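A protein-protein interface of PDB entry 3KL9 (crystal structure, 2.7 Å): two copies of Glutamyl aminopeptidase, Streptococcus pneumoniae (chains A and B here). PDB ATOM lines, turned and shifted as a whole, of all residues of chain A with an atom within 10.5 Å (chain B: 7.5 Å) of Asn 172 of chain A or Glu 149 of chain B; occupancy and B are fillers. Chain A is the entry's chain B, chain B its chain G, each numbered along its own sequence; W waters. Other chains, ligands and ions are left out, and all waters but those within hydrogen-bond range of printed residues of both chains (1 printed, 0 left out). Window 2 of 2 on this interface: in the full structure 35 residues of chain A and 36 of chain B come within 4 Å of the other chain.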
ATOM      1  N   ILE A 168       8.478  22.064   5.586  1.00  0.00           N
ATOM      2  CA  ILE A 168       9.928  21.900   5.436  1.00  0.00           C
ATOM      3  C   ILE A 168      10.318  20.504   4.939  1.00  0.00           C
ATOM      4  O   ILE A 168       9.714  19.498   5.335  1.00  0.00           O
ATOM      5  CB  ILE A 168      10.728  22.235   6.752  1.00  0.00           C
ATOM      6  CG1 ILE A 168      10.256  21.375   7.934  1.00  0.00           C
ATOM      7  CG2 ILE A 168      10.654  23.736   7.084  1.00  0.00           C
ATOM      8  CD1 ILE A 168      11.261  21.258   9.063  1.00  0.00           C
ATOM      9  N   LEU A 169      11.325  20.468   4.065  1.00  0.00           N
ATOM     10  CA  LEU A 169      11.970  19.233   3.622  1.00  0.00           C
ATOM     11  C   LEU A 169      12.749  18.556   4.761  1.00  0.00           C
ATOM     12  O   LEU A 169      13.423  19.221   5.553  1.00  0.00           O
ATOM     13  CB  LEU A 169      12.946  19.563   2.489  1.00  0.00           C
ATOM     14  CG  LEU A 169      12.776  19.165   1.014  1.00  0.00           C
ATOM     15  CD1 LEU A 169      11.392  18.641   0.647  1.00  0.00           C
ATOM     16  CD2 LEU A 169      13.184  20.338   0.121  1.00  0.00           C
ATOM     17  N   THR A 170      12.654  17.233   4.836  1.00  0.00           N
ATOM     18  CA  THR A 170      13.493  16.459   5.750  1.00  0.00           C
ATOM     19  C   THR A 170      14.935  16.406   5.238  1.00  0.00           C
ATOM     20  O   THR A 170      15.204  16.800   4.104  1.00  0.00           O
ATOM     21  CB  THR A 170      12.959  15.038   5.961  1.00  0.00           C
ATOM     22  OG1 THR A 170      12.891  14.359   4.703  1.00  0.00           O
ATOM     23  CG2 THR A 170      11.578  15.088   6.580  1.00  0.00           C
ATOM     24  N   ALA A 171      15.849  15.919   6.071  1.00  0.00           N
ATOM     25  CA  ALA A 171      17.271  15.900   5.729  1.00  0.00           C
ATOM     26  C   ALA A 171      17.558  15.280   4.355  1.00  0.00           C
ATOM     27  O   ALA A 171      18.334  15.839   3.572  1.00  0.00           O
ATOM     28  CB  ALA A 171      18.078  15.206   6.812  1.00  0.00           C
ATOM     29  N   ASN A 172      16.929  14.141   4.058  1.00  0.00           N
ATOM     30  CA  ASN A 172      17.176  13.452   2.781  1.00  0.00           C
ATOM     31  C   ASN A 172      16.389  14.031   1.604  1.00  0.00           C
ATOM     32  O   ASN A 172      16.551  13.590   0.463  1.00  0.00           O
ATOM     33  CB  ASN A 172      16.939  11.942   2.902  1.00  0.00           C
ATOM     34  CG  ASN A 172      15.481  11.589   3.069  1.00  0.00           C
ATOM     35  OD1 ASN A 172      14.595  12.431   2.911  1.00  0.00           O
ATOM     36  ND2 ASN A 172      15.222  10.328   3.392  1.00  0.00           N
ATOM     37  N   GLU A 173      15.533  15.007   1.901  1.00  0.00           N
ATOM     38  CA  GLU A 173      14.773  15.750   0.896  1.00  0.00           C
ATOM     39  C   GLU A 173      13.769  14.888   0.141  1.00  0.00           C
ATOM     40  O   GLU A 173      13.261  15.287  -0.909  1.00  0.00           O
ATOM     41  CB  GLU A 173      15.717  16.497  -0.056  1.00  0.00           C
ATOM     42  CG  GLU A 173      16.682  17.428   0.692  1.00  0.00           C
ATOM     43  CD  GLU A 173      17.541  18.283  -0.218  1.00  0.00           C
ATOM     44  OE1 GLU A 173      17.585  18.019  -1.440  1.00  0.00           O
ATOM     45  OE2 GLU A 173      18.177  19.225   0.303  1.00  0.00           O
ATOM     46  N   LYS A 174      13.469  13.719   0.702  1.00  0.00           N
ATOM     47  CA  LYS A 174      12.485  12.807   0.125  1.00  0.00           C
ATOM     48  C   LYS A 174      11.134  12.933   0.827  1.00  0.00           C
ATOM     49  O   LYS A 174      10.099  12.512   0.298  1.00  0.00           O
ATOM     50  CB  LYS A 174      12.987  11.349   0.176  1.00  0.00           C
ATOM     51  CG  LYS A 174      13.927  10.930  -0.967  1.00  0.00           C
ATOM     52  CD  LYS A 174      13.254  11.126  -2.342  1.00  0.00           C
ATOM     53  CE  LYS A 174      13.649  10.046  -3.355  1.00  0.00           C
ATOM     54  NZ  LYS A 174      15.108  10.073  -3.687  1.00  0.00           N
ATOM     55  N   ASN A 175      11.152  13.516   2.021  1.00  0.00           N
ATOM     56  CA  ASN A 175       9.945  13.666   2.814  1.00  0.00           C
ATOM     57  C   ASN A 175       9.705  15.124   3.216  1.00  0.00           C
ATOM     58  O   ASN A 175      10.609  15.963   3.135  1.00  0.00           O
ATOM     59  CB  ASN A 175       9.987  12.745   4.046  1.00  0.00           C
ATOM     60  CG  ASN A 175      10.364  11.296   3.704  1.00  0.00           C
ATOM     61  OD1 ASN A 175       9.787  10.668   2.812  1.00  0.00           O
ATOM     62  ND2 ASN A 175      11.342  10.766   4.425  1.00  0.00           N
ATOM     63  N   ILE A 176       8.476  15.420   3.632  1.00  0.00           N
ATOM     64  CA  ILE A 176       8.098  16.763   4.070  1.00  0.00           C
ATOM     65  C   ILE A 176       7.503  16.719   5.478  1.00  0.00           C
ATOM     66  O   ILE A 176       6.814  15.767   5.845  1.00  0.00           O
ATOM     67  CB  ILE A 176       7.099  17.433   3.078  1.00  0.00           C
ATOM     68  CG1 ILE A 176       7.811  17.775   1.767  1.00  0.00           C
ATOM     69  CG2 ILE A 176       6.502  18.706   3.668  1.00  0.00           C
ATOM     70  CD1 ILE A 176       6.889  18.124   0.612  1.00  0.00           C
ATOM     71  N   ILE A 177       7.802  17.748   6.263  1.00  0.00           N
ATOM     72  CA  ILE A 177       7.103  17.995   7.511  1.00  0.00           C
ATOM     73  C   ILE A 177       6.252  19.260   7.334  1.00  0.00           C
ATOM     74  O   ILE A 177       6.767  20.320   6.949  1.00  0.00           O
ATOM     75  CB  ILE A 177       8.082  18.152   8.712  1.00  0.00           C
ATOM     76  CG1 ILE A 177       8.941  16.893   8.885  1.00  0.00           C
ATOM     77  CG2 ILE A 177       7.321  18.456   9.997  1.00  0.00           C
ATOM     78  CD1 ILE A 177      10.243  17.124   9.626  1.00  0.00           C
ATOM     79  N   LYS A 250       2.561   2.362   5.515  1.00  0.00           N
ATOM     80  CA  LYS A 250       3.997   2.622   5.493  1.00  0.00           C
ATOM     81  C   LYS A 250       4.382   3.703   4.463  1.00  0.00           C
ATOM     82  O   LYS A 250       4.190   3.532   3.256  1.00  0.00           O
ATOM     83  CB  LYS A 250       4.731   1.297   5.261  1.00  0.00           C
ATOM     84  CG  LYS A 250       6.246   1.345   5.233  1.00  0.00           C
ATOM     85  CD  LYS A 250       6.803  -0.092   5.171  1.00  0.00           C
ATOM     86  CE  LYS A 250       8.160  -0.186   4.454  1.00  0.00           C
ATOM     87  NZ  LYS A 250       9.285   0.390   5.234  1.00  0.00           N
ATOM     88  N   ILE A 251       4.888   4.827   4.975  1.00  0.00           N
ATOM     89  CA  ILE A 251       5.450   5.939   4.194  1.00  0.00           C
ATOM     90  C   ILE A 251       6.402   5.453   3.104  1.00  0.00           C
ATOM     91  O   ILE A 251       7.380   4.779   3.389  1.00  0.00           O
ATOM     92  CB  ILE A 251       6.163   6.964   5.157  1.00  0.00           C
ATOM     93  CG1 ILE A 251       5.240   8.122   5.517  1.00  0.00           C
ATOM     94  CG2 ILE A 251       7.408   7.581   4.553  1.00  0.00           C
ATOM     95  CD1 ILE A 251       3.810   7.738   5.706  1.00  0.00           C
ATOM     96  N   GLY A 252       6.098   5.783   1.854  1.00  0.00           N
ATOM     97  CA  GLY A 252       6.950   5.411   0.731  1.00  0.00           C
ATOM     98  C   GLY A 252       6.625   4.066   0.112  1.00  0.00           C
ATOM     99  O   GLY A 252       7.339   3.612  -0.773  1.00  0.00           O
ATOM    100  N   ARG A 316       2.490  10.102   8.542  1.00  0.00           N
ATOM    101  CA  ARG A 316       2.727   9.915   9.958  1.00  0.00           C
ATOM    102  C   ARG A 316       2.177  11.095  10.726  1.00  0.00           C
ATOM    103  O   ARG A 316       2.318  12.244  10.299  1.00  0.00           O
ATOM    104  CB  ARG A 316       4.217   9.746  10.239  1.00  0.00           C
ATOM    105  CG  ARG A 316       4.851   8.645   9.437  1.00  0.00           C
ATOM    106  CD  ARG A 316       6.270   8.413   9.876  1.00  0.00           C
ATOM    107  NE  ARG A 316       6.853   7.245   9.217  1.00  0.00           N
ATOM    108  CZ  ARG A 316       8.156   7.060   9.038  1.00  0.00           C
ATOM    109  NH1 ARG A 316       9.027   7.970   9.456  1.00  0.00           N
ATOM    110  NH2 ARG A 316       8.582   5.973   8.422  1.00  0.00           N
ATOM    111  N   LEU A 324       4.344  13.986   8.808  1.00  0.00           N
ATOM    112  CA  LEU A 324       5.479  13.589   7.990  1.00  0.00           C
ATOM    113  C   LEU A 324       5.023  12.598   6.931  1.00  0.00           C
ATOM    114  O   LEU A 324       4.315  11.641   7.228  1.00  0.00           O
ATOM    115  CB  LEU A 324       6.576  12.975   8.860  1.00  0.00           C
ATOM    116  CG  LEU A 324       8.010  12.907   8.307  1.00  0.00           C
ATOM    117  CD1 LEU A 324       9.015  12.833   9.451  1.00  0.00           C
ATOM    118  CD2 LEU A 324       8.216  11.745   7.340  1.00  0.00           C
ATOM    119  N   TYR A 325       5.446  12.835   5.697  1.00  0.00           N
ATOM    120  CA  TYR A 325       4.967  12.076   4.549  1.00  0.00           C
ATOM    121  C   TYR A 325       5.951  12.179   3.388  1.00  0.00           C
ATOM    122  O   TYR A 325       6.778  13.096   3.351  1.00  0.00           O
ATOM    123  CB  TYR A 325       3.589  12.590   4.113  1.00  0.00           C
ATOM    124  CG  TYR A 325       3.510  14.088   3.931  1.00  0.00           C
ATOM    125  CD1 TYR A 325       3.580  14.660   2.664  1.00  0.00           C
ATOM    126  CD2 TYR A 325       3.363  14.933   5.029  1.00  0.00           C
ATOM    127  CE1 TYR A 325       3.505  16.041   2.492  1.00  0.00           C
ATOM    128  CE2 TYR A 325       3.294  16.317   4.871  1.00  0.00           C
ATOM    129  CZ  TYR A 325       3.359  16.863   3.599  1.00  0.00           C
ATOM    130  OH  TYR A 325       3.281  18.228   3.450  1.00  0.00           O
ATOM    131  N   ALA A 326       5.844  11.245   2.439  1.00  0.00           N
ATOM    132  CA  ALA A 326       6.773  11.137   1.310  1.00  0.00           C
ATOM    133  C   ALA A 326       6.190  11.735   0.041  1.00  0.00           C
ATOM    134  O   ALA A 326       5.057  11.437  -0.322  1.00  0.00           O
ATOM    135  CB  ALA A 326       7.143   9.676   1.078  1.00  0.00           C
ATOM    136  N   MET A 327       6.977  12.566  -0.642  1.00  0.00           N
ATOM    137  CA  MET A 327       6.576  13.138  -1.934  1.00  0.00           C
ATOM    138  C   MET A 327       6.322  12.043  -2.953  1.00  0.00           C
ATOM    139  O   MET A 327       5.375  12.112  -3.724  1.00  0.00           O
ATOM    140  CB  MET A 327       7.643  14.101  -2.462  1.00  0.00           C
ATOM    141  CG  MET A 327       7.665  15.435  -1.747  1.00  0.00           C
ATOM    142  SD  MET A 327       8.847  16.591  -2.441  1.00  0.00           S
ATOM    143  CE  MET A 327      10.386  15.855  -1.907  1.00  0.00           C
ATOM    144  N   ASP A 328       7.183  11.033  -2.933  1.00  0.00           N
ATOM    145  CA  ASP A 328       7.073   9.847  -3.773  1.00  0.00           C
ATOM    146  C   ASP A 328       5.683   9.232  -3.746  1.00  0.00           C
ATOM    147  O   ASP A 328       5.151   8.819  -4.784  1.00  0.00           O
ATOM    148  CB  ASP A 328       8.066   8.806  -3.281  1.00  0.00           C
ATOM    149  CG  ASP A 328       8.651   7.999  -4.403  1.00  0.00           C
ATOM    150  OD1 ASP A 328       9.884   8.129  -4.605  1.00  0.00           O
ATOM    151  OD2 ASP A 328       7.885   7.247  -5.077  1.00  0.00           O
ATOM    152  N   ILE B  78      19.195   4.972  18.155  1.00  0.00           N
ATOM    153  CA  ILE B  78      18.599   5.027  16.818  1.00  0.00           C
ATOM    154  C   ILE B  78      18.018   3.656  16.505  1.00  0.00           C
ATOM    155  O   ILE B  78      18.743   2.672  16.418  1.00  0.00           O
ATOM    156  CB  ILE B  78      19.626   5.408  15.709  1.00  0.00           C
ATOM    157  CG1 ILE B  78      20.514   6.579  16.148  1.00  0.00           C
ATOM    158  CG2 ILE B  78      18.906   5.715  14.401  1.00  0.00           C
ATOM    159  CD1 ILE B  78      21.643   6.920  15.188  1.00  0.00           C
ATOM    160  N   PRO B  80      16.163   0.552  14.382  1.00  0.00           N
ATOM    161  CA  PRO B  80      16.539   0.094  13.031  1.00  0.00           C
ATOM    162  C   PRO B  80      15.748   0.777  11.918  1.00  0.00           C
ATOM    163  O   PRO B  80      16.222   0.827  10.784  1.00  0.00           O
ATOM    164  CB  PRO B  80      16.256  -1.420  13.053  1.00  0.00           C
ATOM    165  CG  PRO B  80      16.224  -1.798  14.503  1.00  0.00           C
ATOM    166  CD  PRO B  80      15.701  -0.564  15.235  1.00  0.00           C
ATOM    167  N   ASP B  81      14.576   1.318  12.247  1.00  0.00           N
ATOM    168  CA  ASP B  81      13.722   1.969  11.254  1.00  0.00           C
ATOM    169  C   ASP B  81      14.023   3.462  11.057  1.00  0.00           C
ATOM    170  O   ASP B  81      13.255   4.182  10.402  1.00  0.00           O
ATOM    171  CB  ASP B  81      12.238   1.743  11.588  1.00  0.00           C
ATOM    172  CG  ASP B  81      11.773   2.538  12.799  1.00  0.00           C
ATOM    173  OD1 ASP B  81      12.617   2.903  13.649  1.00  0.00           O
ATOM    174  OD2 ASP B  81      10.554   2.803  12.895  1.00  0.00           O
ATOM    175  N   GLY B  82      15.131   3.923  11.631  1.00  0.00           N
ATOM    176  CA  GLY B  82      15.603   5.299  11.416  1.00  0.00           C
ATOM    177  C   GLY B  82      14.984   6.377  12.287  1.00  0.00           C
ATOM    178  O   GLY B  82      15.222   7.578  12.072  1.00  0.00           O
ATOM    179  N   ILE B 112      19.675  18.649  11.453  1.00  0.00           N
ATOM    180  CA  ILE B 112      18.661  17.838  10.802  1.00  0.00           C
ATOM    181  C   ILE B 112      17.259  18.014  11.428  1.00  0.00           C
ATOM    182  O   ILE B 112      17.084  17.854  12.634  1.00  0.00           O
ATOM    183  CB  ILE B 112      19.117  16.333  10.591  1.00  0.00           C
ATOM    184  CG1 ILE B 112      18.573  15.398  11.656  1.00  0.00           C
ATOM    185  CG2 ILE B 112      20.623  16.177  10.408  1.00  0.00           C
ATOM    186  CD1 ILE B 112      17.382  14.603  11.129  1.00  0.00           C
ATOM    187  N   PRO B 113      16.264  18.392  10.608  1.00  0.00           N
ATOM    188  CA  PRO B 113      14.907  18.577  11.108  1.00  0.00           C
ATOM    189  C   PRO B 113      14.351  17.291  11.704  1.00  0.00           C
ATOM    190  O   PRO B 113      14.333  16.252  11.042  1.00  0.00           O
ATOM    191  CB  PRO B 113      14.122  18.968   9.855  1.00  0.00           C
ATOM    192  CG  PRO B 113      15.116  19.570   8.967  1.00  0.00           C
ATOM    193  CD  PRO B 113      16.383  18.812   9.201  1.00  0.00           C
ATOM    194  N   GLY B 142      13.153  11.827  11.903  1.00  0.00           N
ATOM    195  CA  GLY B 142      13.871  12.705  10.987  1.00  0.00           C
ATOM    196  C   GLY B 142      13.588  12.378   9.532  1.00  0.00           C
ATOM    197  O   GLY B 142      14.253  12.899   8.632  1.00  0.00           O
ATOM    198  N   GLY B 143      12.603  11.505   9.312  1.00  0.00           N
ATOM    199  CA  GLY B 143      12.172  11.094   7.974  1.00  0.00           C
ATOM    200  C   GLY B 143      13.164  10.207   7.244  1.00  0.00           C
ATOM    201  O   GLY B 143      13.444  10.421   6.060  1.00  0.00           O
ATOM    202  N   PHE B 144      13.701   9.211   7.947  1.00  0.00           N
ATOM    203  CA  PHE B 144      14.704   8.318   7.370  1.00  0.00           C
ATOM    204  C   PHE B 144      14.127   6.927   7.118  1.00  0.00           C
ATOM    205  O   PHE B 144      13.157   6.524   7.770  1.00  0.00           O
ATOM    206  CB  PHE B 144      15.947   8.236   8.267  1.00  0.00           C
ATOM    207  CG  PHE B 144      16.667   9.544   8.431  1.00  0.00           C
ATOM    208  CD1 PHE B 144      16.620  10.225   9.637  1.00  0.00           C
ATOM    209  CD2 PHE B 144      17.401  10.094   7.378  1.00  0.00           C
ATOM    210  CE1 PHE B 144      17.286  11.447   9.801  1.00  0.00           C
ATOM    211  CE2 PHE B 144      18.071  11.322   7.528  1.00  0.00           C
ATOM    212  CZ  PHE B 144      18.016  11.998   8.744  1.00  0.00           C
ATOM    213  N   ALA B 145      14.727   6.210   6.167  1.00  0.00           N
ATOM    214  CA  ALA B 145      14.285   4.868   5.787  1.00  0.00           C
ATOM    215  C   ALA B 145      14.717   3.814   6.800  1.00  0.00           C
ATOM    216  O   ALA B 145      13.987   2.845   7.036  1.00  0.00           O
ATOM    217  CB  ALA B 145      14.802   4.505   4.396  1.00  0.00           C
ATOM    218  N   ASP B 146      15.905   4.005   7.385  1.00  0.00           N
ATOM    219  CA  ASP B 146      16.463   3.061   8.364  1.00  0.00           C
ATOM    220  C   ASP B 146      17.556   3.655   9.242  1.00  0.00           C
ATOM    221  O   ASP B 146      17.963   4.800   9.056  1.00  0.00           O
ATOM    222  CB  ASP B 146      16.979   1.775   7.688  1.00  0.00           C
ATOM    223  CG  ASP B 146      17.778   2.041   6.418  1.00  0.00           C
ATOM    224  OD1 ASP B 146      17.549   1.305   5.445  1.00  0.00           O
ATOM    225  OD2 ASP B 146      18.622   2.965   6.377  1.00  0.00           O
ATOM    226  N   LYS B 147      18.009   2.859  10.209  1.00  0.00           N
ATOM    227  CA  LYS B 147      19.181   3.170  11.027  1.00  0.00           C
ATOM    228  C   LYS B 147      20.371   3.607  10.163  1.00  0.00           C
ATOM    229  O   LYS B 147      20.982   4.646  10.421  1.00  0.00           O
ATOM    230  CB  LYS B 147      19.544   1.967  11.908  1.00  0.00           C
ATOM    231  CG  LYS B 147      20.827   2.107  12.716  1.00  0.00           C
ATOM    232  CD  LYS B 147      20.654   1.536  14.129  1.00  0.00           C
ATOM    233  CE  LYS B 147      21.905   0.838  14.653  1.00  0.00           C
ATOM    234  NZ  LYS B 147      23.065   1.749  14.764  1.00  0.00           N
ATOM    235  N   ALA B 148      20.672   2.828   9.126  1.00  0.00           N
ATOM    236  CA  ALA B 148      21.789   3.136   8.230  1.00  0.00           C
ATOM    237  C   ALA B 148      21.724   4.550   7.651  1.00  0.00           C
ATOM    238  O   ALA B 148      22.713   5.286   7.701  1.00  0.00           O
ATOM    239  CB  ALA B 148      21.896   2.091   7.109  1.00  0.00           C
ATOM    240  N   GLU B 149      20.568   4.935   7.114  1.00  0.00           N
ATOM    241  CA  GLU B 149      20.450   6.249   6.499  1.00  0.00           C
ATOM    242  C   GLU B 149      20.638   7.355   7.531  1.00  0.00           C
ATOM    243  O   GLU B 149      21.417   8.290   7.307  1.00  0.00           O
ATOM    244  CB  GLU B 149      19.124   6.419   5.768  1.00  0.00           C
ATOM    245  CG  GLU B 149      19.151   7.603   4.817  1.00  0.00           C
ATOM    246  CD  GLU B 149      17.806   7.912   4.185  1.00  0.00           C
ATOM    247  OE1 GLU B 149      17.806   8.466   3.061  1.00  0.00           O
ATOM    248  OE2 GLU B 149      16.754   7.618   4.801  1.00  0.00           O
ATOM    249  N   ALA B 150      19.940   7.236   8.661  1.00  0.00           N
ATOM    250  CA  ALA B 150      20.067   8.193   9.756  1.00  0.00           C
ATOM    251  C   ALA B 150      21.538   8.469  10.070  1.00  0.00           C
ATOM    252  O   ALA B 150      21.952   9.624  10.179  1.00  0.00           O
ATOM    253  CB  ALA B 150      19.343   7.691  10.993  1.00  0.00           C
ATOM    254  N   GLU B 151      22.326   7.407  10.181  1.00  0.00           N
ATOM    255  CA  GLU B 151      23.746   7.529  10.496  1.00  0.00           C
ATOM    256  C   GLU B 151      24.583   8.166   9.378  1.00  0.00           C
ATOM    257  O   GLU B 151      25.572   8.848   9.659  1.00  0.00           O
ATOM    258  CB  GLU B 151      24.319   6.170  10.901  1.00  0.00           C
ATOM    259  CG  GLU B 151      23.713   5.604  12.184  1.00  0.00           C
ATOM    260  CD  GLU B 151      24.308   4.268  12.580  1.00  0.00           C
ATOM    261  OE1 GLU B 151      24.266   3.936  13.784  1.00  0.00           O
ATOM    262  OE2 GLU B 151      24.818   3.550  11.693  1.00  0.00           O
ATOM    263  N   SER B 152      24.185   7.957   8.124  1.00  0.00           N
ATOM    264  CA  SER B 152      24.928   8.508   6.985  1.00  0.00           C
ATOM    265  C   SER B 152      24.858  10.038   6.943  1.00  0.00           C
ATOM    266  O   SER B 152      25.692  10.684   6.311  1.00  0.00           O
ATOM    267  CB  SER B 152      24.446   7.908   5.663  1.00  0.00           C
ATOM    268  OG  SER B 152      23.152   8.375   5.321  1.00  0.00           O
ATOM    269  N   PHE B 153      23.864  10.606   7.623  1.00  0.00           N
ATOM    270  CA  PHE B 153      23.751  12.057   7.772  1.00  0.00           C
ATOM    271  C   PHE B 153      24.495  12.565   9.008  1.00  0.00           C
ATOM    272  O   PHE B 153      24.316  13.711   9.423  1.00  0.00           O
ATOM    273  CB  PHE B 153      22.281  12.478   7.809  1.00  0.00           C
ATOM    274  CG  PHE B 153      21.661  12.614   6.450  1.00  0.00           C
ATOM    275  CD1 PHE B 153      21.170  11.494   5.774  1.00  0.00           C
ATOM    276  CD2 PHE B 153      21.577  13.865   5.831  1.00  0.00           C
ATOM    277  CE1 PHE B 153      20.599  11.615   4.504  1.00  0.00           C
ATOM    278  CE2 PHE B 153      21.013  13.995   4.549  1.00  0.00           C
ATOM    279  CZ  PHE B 153      20.523  12.866   3.888  1.00  0.00           C
ATOM    280  N   GLY B 154      25.326  11.700   9.589  1.00  0.00           N
ATOM    281  CA  GLY B 154      26.195  12.059  10.708  1.00  0.00           C
ATOM    282  C   GLY B 154      25.565  11.958  12.085  1.00  0.00           C
ATOM    283  O   GLY B 154      26.098  12.507  13.048  1.00  0.00           O
ATOM    284  N   ILE B 155      24.438  11.255  12.177  1.00  0.00           N
ATOM    285  CA  ILE B 155      23.671  11.166  13.422  1.00  0.00           C
ATOM    286  C   ILE B 155      24.181  10.047  14.336  1.00  0.00           C
ATOM    287  O   ILE B 155      24.417   8.924  13.894  1.00  0.00           O
ATOM    288  CB  ILE B 155      22.156  10.993  13.148  1.00  0.00           C
ATOM    289  CG1 ILE B 155      21.592  12.239  12.447  1.00  0.00           C
ATOM    290  CG2 ILE B 155      21.392  10.689  14.445  1.00  0.00           C
ATOM    291  CD1 ILE B 155      20.224  12.035  11.842  1.00  0.00           C
ATOM    292  N   ARG B 156      24.350  10.373  15.615  1.00  0.00           N
ATOM    293  CA  ARG B 156      24.884   9.428  16.585  1.00  0.00           C
ATOM    294  C   ARG B 156      24.168   9.542  17.919  1.00  0.00           C
ATOM    295  O   ARG B 156      23.673  10.612  18.272  1.00  0.00           O
ATOM    296  CB  ARG B 156      26.382   9.667  16.802  1.00  0.00           C
ATOM    297  CG  ARG B 156      27.278   9.331  15.615  1.00  0.00           C
ATOM    298  CD  ARG B 156      27.237   7.854  15.246  1.00  0.00           C
ATOM    299  NE  ARG B 156      28.096   7.570  14.099  1.00  0.00           N
ATOM    300  CZ  ARG B 156      27.789   7.826  12.824  1.00  0.00           C
ATOM    301  NH1 ARG B 156      26.626   8.382  12.496  1.00  0.00           N
ATOM    302  NH2 ARG B 156      28.657   7.524  11.868  1.00  0.00           N
HETATM  303  O   HOH W   1      10.937   4.207   9.134  1.00  0.00           O
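Among the printed residues, pairs that only touch across the chains: Ile 168 of chain A with Pro 113 of chain B (3.7 Å), Leu 169 of chain A with Pro 113 of chain B (3.8 Å), Thr 170 of chain A with Gly 142 of chain B (3.7 Å), Ala 171 of chain A with Phe 144 of chain B (3.7 Å), Ala 171 of chain A with Phe 153 of chain B (3.4 Å), Asn 172 of chain A with Phe 153 of chain B (3.6 Å) and Leu 324 of chain A with Gly 143 of chain B (3.8 Å).
No position is printed for both chains.
Of the 10 pairs that touch across the chains among the printed residues, none has its exchanged pair printed and touching as well.
The side-chain amide oxygen of Asn 172 of chain A sits at hydrogen-bond distance from the backbone NH of Lys 174 of chain A (2.8 Å).
OD1 of Asn 172 of chain A sits at hydrogen-bond distance from OG1 of Thr 170 of chain A (3.1 Å).
N of Arg 316 of chain A lies within hydrogen-bond range of O of Leu 324 of chain A (2.7 Å).
The backbone carbonyl oxygen (O) of Ile 168 of chain A lies within hydrogen-bond range of the backbone NH (N) of Ile 177 of chain A, 2.8 Å away.
The backbone carbonyl oxygen of Glu 149 of chain B sits at hydrogen-bond distance from the side-chain hydroxyl of Ser 152 of chain B (2.6 Å).
The side-chain carboxylate of Asp 146 of chain B sits at hydrogen-bond distance from the backbone NH of Glu 149 of chain B (2.9 Å).
The backbone carbonyl oxygen (O) of Gly 143 of chain B is in hydrogen-bond range of the side-chain amide nitrogen (ND2) of Asn 172 of chain A, 3.2 Å away.
ND2 of Asn 172 of chain A lies within hydrogen-bond range of OE1 of Glu 149 of chain B, at 3.2 Å.
The backbone carbonyl oxygen (O) of Gly 143 of chain B sits at hydrogen-bond distance from the side-chain amide nitrogen (ND2) of Asn 175 of chain A (2.7 Å).
Of the printed residues of chain B, Thr 170 of chain A touches Gly 142.
Of chain B, only Phe 144 (3.7 Å) and Phe 153 (3.4 Å) come within 4 Å of Ala 171 of chain A.
Of chain B, only Gly 143 (3.2 Å), Glu 149 (3.2 Å) and Phe 153 (3.6 Å) come within 4 Å of Asn 172 of chain A.
Printed residues of chain B within 4 Å of Leu 324 of chain A: Gly 143.
Printed residues of chain A within 4 Å of Pro 113 of chain B: Ile 168 and Leu 169.
Of the printed residues of chain A, Gly 143 of chain B touches Asn 172 (3.2 Å), Asn 175 (2.7 Å) and Leu 324 (3.8 Å).
Phe 144 of chain B touches just one residue of chain A: Ala 171.
No residue of chain A comes within 4 Å of Ala 145 of chain B.
Asp 146 of chain B touches none of the printed residues of chain A.
Ala 148 of chain B touches none of the printed residues of chain A.
No residue of chain A comes within 4 Å of Ala 150 of chain B.
No residue of chain A comes within 4 Å of Ser 152 of chain B.
The nearest residue of chain B that does not touch Asn 172 of chain A is Phe 144 of chain B (4.5 Å).
Printed residues of chain A that touch a printed residue of chain B: Ile 168, Leu 169, Thr 170, Ala 171, Asn 172, Asn 175 and Leu 324.
Hydrophobic or aromatic side chains of chain A within 4 Å of the printed part of chain B: Ile 168, Ala 171 and Leu 324.
Among the printed residues, no Asp or Glu carboxylate lies within 4 Å of a Lys or Arg side-chain nitrogen of the other chain.
Water W1 lies within hydrogen-bond range of the backbone carbonyl oxygen (O) of Asp 81 of chain B, the guanidinium group (NH2) of Arg 316 of chain A and the backbone carbonyl oxygen (O) of Phe 144 of chain B.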
